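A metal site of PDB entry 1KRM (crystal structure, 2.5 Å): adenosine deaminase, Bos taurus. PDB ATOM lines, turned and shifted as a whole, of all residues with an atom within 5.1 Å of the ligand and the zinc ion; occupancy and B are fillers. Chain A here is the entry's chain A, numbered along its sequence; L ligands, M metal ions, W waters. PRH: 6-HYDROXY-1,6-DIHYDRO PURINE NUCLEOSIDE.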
ATOM      1  N   HIS A  14      33.262 -10.491  36.528  1.00  0.00           N
ATOM      2  CA  HIS A  14      32.448 -10.250  35.314  1.00  0.00           C
ATOM      3  C   HIS A  14      31.822 -11.485  34.688  1.00  0.00           C
ATOM      4  O   HIS A  14      32.437 -12.146  33.853  1.00  0.00           O
ATOM      5  CB  HIS A  14      33.222  -9.467  34.197  1.00  0.00           C
ATOM      6  CG  HIS A  14      32.410  -8.786  33.077  1.00  0.00           C
ATOM      7  ND1 HIS A  14      32.322  -7.460  32.949  1.00  0.00           N
ATOM      8  CD2 HIS A  14      31.758  -9.336  31.945  1.00  0.00           C
ATOM      9  CE1 HIS A  14      31.674  -7.190  31.776  1.00  0.00           C
ATOM     10  NE2 HIS A  14      31.294  -8.347  31.136  1.00  0.00           N
ATOM     11  N   HIS A  16      27.884 -13.084  32.940  1.00  0.00           N
ATOM     12  CA  HIS A  16      26.470 -12.821  32.844  1.00  0.00           C
ATOM     13  C   HIS A  16      25.586 -14.072  32.983  1.00  0.00           C
ATOM     14  O   HIS A  16      25.598 -14.957  32.123  1.00  0.00           O
ATOM     15  CB  HIS A  16      26.191 -12.053  31.527  1.00  0.00           C
ATOM     16  CG  HIS A  16      26.964 -10.724  31.335  1.00  0.00           C
ATOM     17  ND1 HIS A  16      26.375  -9.583  30.968  1.00  0.00           N
ATOM     18  CD2 HIS A  16      28.338 -10.458  31.326  1.00  0.00           C
ATOM     19  CE1 HIS A  16      27.307  -8.642  30.728  1.00  0.00           C
ATOM     20  NE2 HIS A  16      28.544  -9.173  30.922  1.00  0.00           N
ATOM     21  N   ASP A  18      22.356 -14.603  32.062  1.00  0.00           N
ATOM     22  CA  ASP A  18      22.107 -14.564  30.613  1.00  0.00           C
ATOM     23  C   ASP A  18      22.784 -15.590  29.744  1.00  0.00           C
ATOM     24  O   ASP A  18      22.106 -16.323  29.088  1.00  0.00           O
ATOM     25  CB  ASP A  18      22.629 -13.210  30.193  1.00  0.00           C
ATOM     26  CG  ASP A  18      21.492 -12.233  30.006  1.00  0.00           C
ATOM     27  OD1 ASP A  18      20.665 -12.026  30.905  1.00  0.00           O
ATOM     28  OD2 ASP A  18      21.445 -11.679  28.914  1.00  0.00           O
ATOM     29  N   LEU A  57      31.123  -7.460  18.076  1.00  0.00           N
ATOM     30  CA  LEU A  57      30.214  -7.247  19.205  1.00  0.00           C
ATOM     31  C   LEU A  57      28.729  -7.194  18.888  1.00  0.00           C
ATOM     32  O   LEU A  57      27.930  -7.879  19.544  1.00  0.00           O
ATOM     33  CB  LEU A  57      30.583  -5.975  19.972  1.00  0.00           C
ATOM     34  CG  LEU A  57      29.711  -5.790  21.219  1.00  0.00           C
ATOM     35  CD1 LEU A  57      30.315  -6.622  22.334  1.00  0.00           C
ATOM     36  CD2 LEU A  57      29.428  -4.331  21.617  1.00  0.00           C
ATOM     37  N   PHE A  60      27.735 -10.916  18.312  1.00  0.00           N
ATOM     38  CA  PHE A  60      27.674 -11.543  19.673  1.00  0.00           C
ATOM     39  C   PHE A  60      26.289 -11.478  20.322  1.00  0.00           C
ATOM     40  O   PHE A  60      25.663 -12.480  20.661  1.00  0.00           O
ATOM     41  CB  PHE A  60      28.763 -10.962  20.636  1.00  0.00           C
ATOM     42  CG  PHE A  60      28.638 -11.429  22.081  1.00  0.00           C
ATOM     43  CD1 PHE A  60      29.055 -12.717  22.466  1.00  0.00           C
ATOM     44  CD2 PHE A  60      28.063 -10.568  23.030  1.00  0.00           C
ATOM     45  CE1 PHE A  60      28.793 -13.174  23.768  1.00  0.00           C
ATOM     46  CE2 PHE A  60      27.826 -11.013  24.344  1.00  0.00           C
ATOM     47  CZ  PHE A  60      28.170 -12.327  24.689  1.00  0.00           C
ATOM     48  N   LEU A  61      25.843 -10.200  20.362  1.00  0.00           N
ATOM     49  CA  LEU A  61      24.657  -9.712  21.077  1.00  0.00           C
ATOM     50  C   LEU A  61      23.273 -10.122  20.629  1.00  0.00           C
ATOM     51  O   LEU A  61      22.269  -9.892  21.316  1.00  0.00           O
ATOM     52  CB  LEU A  61      24.774  -8.183  21.184  1.00  0.00           C
ATOM     53  CG  LEU A  61      25.613  -7.993  22.403  1.00  0.00           C
ATOM     54  CD1 LEU A  61      26.697  -6.964  22.253  1.00  0.00           C
ATOM     55  CD2 LEU A  61      24.715  -7.820  23.573  1.00  0.00           C
ATOM     56  N   PHE A  64      22.269 -14.411  21.418  1.00  0.00           N
ATOM     57  CA  PHE A  64      21.198 -14.290  22.407  1.00  0.00           C
ATOM     58  C   PHE A  64      19.758 -14.368  21.991  1.00  0.00           C
ATOM     59  O   PHE A  64      18.889 -14.710  22.775  1.00  0.00           O
ATOM     60  CB  PHE A  64      21.311 -12.981  23.146  1.00  0.00           C
ATOM     61  CG  PHE A  64      22.432 -13.020  24.125  1.00  0.00           C
ATOM     62  CD1 PHE A  64      23.765 -12.976  23.669  1.00  0.00           C
ATOM     63  CD2 PHE A  64      22.117 -13.085  25.483  1.00  0.00           C
ATOM     64  CE1 PHE A  64      24.827 -12.989  24.579  1.00  0.00           C
ATOM     65  CE2 PHE A  64      23.172 -13.069  26.386  1.00  0.00           C
ATOM     66  CZ  PHE A  64      24.503 -13.035  25.932  1.00  0.00           C
ATOM     67  N   ARG A 100      26.282 -10.710  37.015  1.00  0.00           N
ATOM     68  CA  ARG A 100      25.315  -9.734  36.513  1.00  0.00           C
ATOM     69  C   ARG A 100      24.228 -10.274  35.644  1.00  0.00           C
ATOM     70  O   ARG A 100      24.359 -11.285  34.987  1.00  0.00           O
ATOM     71  CB  ARG A 100      25.967  -8.537  35.801  1.00  0.00           C
ATOM     72  CG  ARG A 100      26.663  -8.811  34.449  1.00  0.00           C
ATOM     73  CD  ARG A 100      27.731  -7.753  34.124  1.00  0.00           C
ATOM     74  NE  ARG A 100      28.660  -7.665  35.246  1.00  0.00           N
ATOM     75  CZ  ARG A 100      29.812  -6.980  35.195  1.00  0.00           C
ATOM     76  NH1 ARG A 100      30.626  -7.142  36.225  1.00  0.00           N
ATOM     77  NH2 ARG A 100      30.159  -6.197  34.214  1.00  0.00           N
ATOM     78  N   TYR A 101      23.144  -9.506  35.645  1.00  0.00           N
ATOM     79  CA  TYR A 101      22.033  -9.799  34.719  1.00  0.00           C
ATOM     80  C   TYR A 101      21.074  -8.656  34.411  1.00  0.00           C
ATOM     81  O   TYR A 101      21.167  -7.547  34.915  1.00  0.00           O
ATOM     82  CB  TYR A 101      21.237 -11.085  35.041  1.00  0.00           C
ATOM     83  CG  TYR A 101      20.414 -11.014  36.311  1.00  0.00           C
ATOM     84  CD1 TYR A 101      19.033 -10.718  36.261  1.00  0.00           C
ATOM     85  CD2 TYR A 101      21.063 -11.268  37.533  1.00  0.00           C
ATOM     86  CE1 TYR A 101      18.343 -10.567  37.457  1.00  0.00           C
ATOM     87  CE2 TYR A 101      20.358 -11.137  38.726  1.00  0.00           C
ATOM     88  CZ  TYR A 101      19.046 -10.698  38.651  1.00  0.00           C
ATOM     89  OH  TYR A 101      18.478 -10.323  39.828  1.00  0.00           O
ATOM     90  N   SER A 102      20.126  -8.949  33.535  1.00  0.00           N
ATOM     91  CA  SER A 102      19.214  -7.870  33.139  1.00  0.00           C
ATOM     92  C   SER A 102      17.720  -8.113  33.317  1.00  0.00           C
ATOM     93  O   SER A 102      17.087  -8.569  32.387  1.00  0.00           O
ATOM     94  CB  SER A 102      19.411  -7.520  31.681  1.00  0.00           C
ATOM     95  OG  SER A 102      18.542  -6.419  31.334  1.00  0.00           O
ATOM     96  N   LEU A 105      15.596  -8.095  30.274  1.00  0.00           N
ATOM     97  CA  LEU A 105      15.426  -9.275  29.392  1.00  0.00           C
ATOM     98  C   LEU A 105      14.521 -10.488  29.845  1.00  0.00           C
ATOM     99  O   LEU A 105      14.036 -11.340  29.106  1.00  0.00           O
ATOM    100  CB  LEU A 105      16.811  -9.680  29.035  1.00  0.00           C
ATOM    101  CG  LEU A 105      17.693  -8.587  28.496  1.00  0.00           C
ATOM    102  CD1 LEU A 105      18.896  -9.270  27.868  1.00  0.00           C
ATOM    103  CD2 LEU A 105      17.008  -7.765  27.391  1.00  0.00           C
ATOM    104  N   CYS A 152      21.742  -4.972  35.731  1.00  0.00           N
ATOM    105  CA  CYS A 152      22.352  -4.267  34.620  1.00  0.00           C
ATOM    106  C   CYS A 152      21.420  -3.367  33.920  1.00  0.00           C
ATOM    107  O   CYS A 152      20.572  -3.837  33.180  1.00  0.00           O
ATOM    108  CB  CYS A 152      22.669  -5.176  33.476  1.00  0.00           C
ATOM    109  SG  CYS A 152      24.360  -5.538  33.477  1.00  0.00           S
ATOM    110  N   MET A 154      20.767  -1.228  30.637  1.00  0.00           N
ATOM    111  CA  MET A 154      21.075  -1.859  29.371  1.00  0.00           C
ATOM    112  C   MET A 154      21.130  -0.816  28.261  1.00  0.00           C
ATOM    113  O   MET A 154      20.092  -0.164  28.041  1.00  0.00           O
ATOM    114  CB  MET A 154      19.898  -2.759  29.236  1.00  0.00           C
ATOM    115  CG  MET A 154      19.997  -3.715  28.111  1.00  0.00           C
ATOM    116  SD  MET A 154      20.849  -5.138  28.697  1.00  0.00           S
ATOM    117  CE  MET A 154      20.457  -5.928  27.151  1.00  0.00           C
ATOM    118  N   ALA A 182      25.133  -2.305  30.121  1.00  0.00           N
ATOM    119  CA  ALA A 182      25.610  -3.386  29.216  1.00  0.00           C
ATOM    120  C   ALA A 182      24.952  -3.504  27.850  1.00  0.00           C
ATOM    121  O   ALA A 182      23.916  -2.908  27.689  1.00  0.00           O
ATOM    122  CB  ALA A 182      25.442  -4.728  29.885  1.00  0.00           C
ATOM    123  N   GLY A 183      25.513  -4.225  26.874  1.00  0.00           N
ATOM    124  CA  GLY A 183      24.895  -4.106  25.536  1.00  0.00           C
ATOM    125  C   GLY A 183      25.854  -3.462  24.537  1.00  0.00           C
ATOM    126  O   GLY A 183      26.982  -3.262  24.943  1.00  0.00           O
ATOM    127  N   HIS A 213      30.388  -1.399  31.378  1.00  0.00           N
ATOM    128  CA  HIS A 213      31.247  -1.970  30.334  1.00  0.00           C
ATOM    129  C   HIS A 213      31.779  -0.960  29.331  1.00  0.00           C
ATOM    130  O   HIS A 213      31.183  -0.713  28.302  1.00  0.00           O
ATOM    131  CB  HIS A 213      30.563  -2.952  29.391  1.00  0.00           C
ATOM    132  CG  HIS A 213      30.103  -4.299  29.923  1.00  0.00           C
ATOM    133  ND1 HIS A 213      29.250  -4.473  30.941  1.00  0.00           N
ATOM    134  CD2 HIS A 213      30.311  -5.543  29.318  1.00  0.00           C
ATOM    135  CE1 HIS A 213      28.927  -5.806  30.959  1.00  0.00           C
ATOM    136  NE2 HIS A 213      29.570  -6.502  29.957  1.00  0.00           N
ATOM    137  N   GLU A 216      36.191  -2.261  25.832  1.00  0.00           N
ATOM    138  CA  GLU A 216      35.789  -3.328  24.873  1.00  0.00           C
ATOM    139  C   GLU A 216      35.815  -2.973  23.376  1.00  0.00           C
ATOM    140  O   GLU A 216      36.892  -2.771  22.844  1.00  0.00           O
ATOM    141  CB  GLU A 216      34.465  -3.962  25.363  1.00  0.00           C
ATOM    142  CG  GLU A 216      33.958  -5.318  24.821  1.00  0.00           C
ATOM    143  CD  GLU A 216      32.523  -5.585  25.239  1.00  0.00           C
ATOM    144  OE1 GLU A 216      31.891  -4.691  25.774  1.00  0.00           O
ATOM    145  OE2 GLU A 216      32.048  -6.680  24.996  1.00  0.00           O
ATOM    146  N   HIS A 237      35.788  -3.807  31.528  1.00  0.00           N
ATOM    147  CA  HIS A 237      36.650  -4.170  30.379  1.00  0.00           C
ATOM    148  C   HIS A 237      37.791  -3.181  30.058  1.00  0.00           C
ATOM    149  O   HIS A 237      38.982  -3.485  30.088  1.00  0.00           O
ATOM    150  CB  HIS A 237      35.965  -4.425  29.039  1.00  0.00           C
ATOM    151  CG  HIS A 237      35.323  -5.765  28.704  1.00  0.00           C
ATOM    152  ND1 HIS A 237      35.960  -6.804  28.146  1.00  0.00           N
ATOM    153  CD2 HIS A 237      33.963  -6.059  28.696  1.00  0.00           C
ATOM    154  CE1 HIS A 237      35.049  -7.710  27.773  1.00  0.00           C
ATOM    155  NE2 HIS A 237      33.805  -7.247  28.124  1.00  0.00           N
ATOM    156  N   ASP A 294      32.763 -13.719  31.518  1.00  0.00           N
ATOM    157  CA  ASP A 294      31.815 -12.985  30.689  1.00  0.00           C
ATOM    158  C   ASP A 294      30.651 -13.795  30.141  1.00  0.00           C
ATOM    159  O   ASP A 294      29.537 -13.690  30.601  1.00  0.00           O
ATOM    160  CB  ASP A 294      32.633 -12.261  29.633  1.00  0.00           C
ATOM    161  CG  ASP A 294      31.993 -11.102  28.908  1.00  0.00           C
ATOM    162  OD1 ASP A 294      31.006 -10.607  29.406  1.00  0.00           O
ATOM    163  OD2 ASP A 294      32.518 -10.694  27.862  1.00  0.00           O
ATOM    164  N   ASP A 295      30.948 -14.646  29.176  1.00  0.00           N
ATOM    165  CA  ASP A 295      29.861 -15.540  28.785  1.00  0.00           C
ATOM    166  C   ASP A 295      30.202 -16.981  28.465  1.00  0.00           C
ATOM    167  O   ASP A 295      30.193 -17.389  27.309  1.00  0.00           O
ATOM    168  CB  ASP A 295      29.158 -15.117  27.515  1.00  0.00           C
ATOM    169  CG  ASP A 295      28.527 -13.786  27.569  1.00  0.00           C
ATOM    170  OD1 ASP A 295      27.301 -13.725  27.491  1.00  0.00           O
ATOM    171  OD2 ASP A 295      29.249 -12.784  27.657  1.00  0.00           O
HETATM  172  N1  PRH L   1      30.067  -6.839  26.653  1.00  0.00           N
HETATM  173  C2  PRH L   1      28.929  -6.400  25.933  1.00  0.00           C
HETATM  174  N3  PRH L   1      27.720  -6.940  26.125  1.00  0.00           N
HETATM  175  C4  PRH L   1      27.774  -8.115  26.919  1.00  0.00           C
HETATM  176  C5  PRH L   1      28.971  -8.703  27.287  1.00  0.00           C
HETATM  177  C6  PRH L   1      30.272  -8.226  26.859  1.00  0.00           C
HETATM  178  O6  PRH L   1      31.118  -8.225  28.047  1.00  0.00           O
HETATM  179  N7  PRH L   1      28.748  -9.752  28.031  1.00  0.00           N
HETATM  180  C8  PRH L   1      27.386  -9.825  28.055  1.00  0.00           C
HETATM  181  N9  PRH L   1      26.774  -8.805  27.430  1.00  0.00           N
HETATM  182  C1' PRH L   1      25.359  -8.365  27.527  1.00  0.00           C
HETATM  183  C2' PRH L   1      24.173  -9.101  26.908  1.00  0.00           C
HETATM  184  O2' PRH L   1      23.332  -8.106  26.170  1.00  0.00           O
HETATM  185  C3' PRH L   1      23.257  -9.367  28.117  1.00  0.00           C
HETATM  186  O3' PRH L   1      21.821  -9.135  27.981  1.00  0.00           O
HETATM  187  C4' PRH L   1      23.677  -8.248  29.014  1.00  0.00           C
HETATM  188  O4' PRH L   1      25.049  -8.406  28.897  1.00  0.00           O
HETATM  189  C5' PRH L   1      23.220  -8.328  30.450  1.00  0.00           C
HETATM  190  O5' PRH L   1      23.612  -9.718  30.903  1.00  0.00           O
HETATM  191 ZN    ZN M   1      30.059  -8.601  29.533  1.00  0.00          ZN
HETATM  192  O   HOH W   1      29.600  -3.013  25.954  1.00  0.00           O
HETATM  193  O   HOH W   2      20.717  -8.384  25.434  1.00  0.00           O
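An oxygen (O6) of the ligand sits close to a ring nitrogen (NE2) of His 237.
The side-chain carboxylate (OD2) of Asp 18 sits at hydrogen-bond distance from an oxygen (O3') of the ligand (2.7 Å).
N1 of the ligand lies within hydrogen-bond range of OE2 of Glu 216.
SD of Met 154 is in hydrogen-bond range of OG of Ser 102, at 3.7 Å.
The guanidinium group (NH2) of Arg 100 is in hydrogen-bond range of a ring nitrogen (ND1) of His 14 (2.8 Å).
N7 of the ligand lies close to OD2 of Asp 295.
Leu 57 touches the ligand.
Phe 60 touches the ligand (CE2 to C4, 3.9 Å).
Leu 61 touches the ligand.
CD1 of Leu 105 touches O3' of the ligand, 2.9 Å away.
Met 154 touches the ligand.
Ala 182 touches the ligand (CB to O4', 3.8 Å).
Gly 183 touches the ligand (N to N3, 3.6 Å).
The nearest printed residue that does not touch the ligand is Phe 64 (4.1 Å).
Four residues have an atom within 4 Å of the zinc ion: His 14, His 16, His 213 and Asp 294.
The zinc ion is bound by an oxygen (O6) of the ligand (1.9 Å), a ring nitrogen (NE2) of His 14 (2.0 Å), a ring nitrogen (NE2) of His 16 (2.1 Å), a ring nitrogen (NE2) of His 213 (2.2 Å), the side-chain carboxylate of Asp 294 (2.2 Å) and a nitrogen (N7) of the ligand (2.3 Å).
The zinc ion has six donor atoms within binding distance.
Water W1 bridges the backbone carbonyl oxygen (O) of Gly 183 and the side-chain carboxylate (OE1) of Glu 216.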
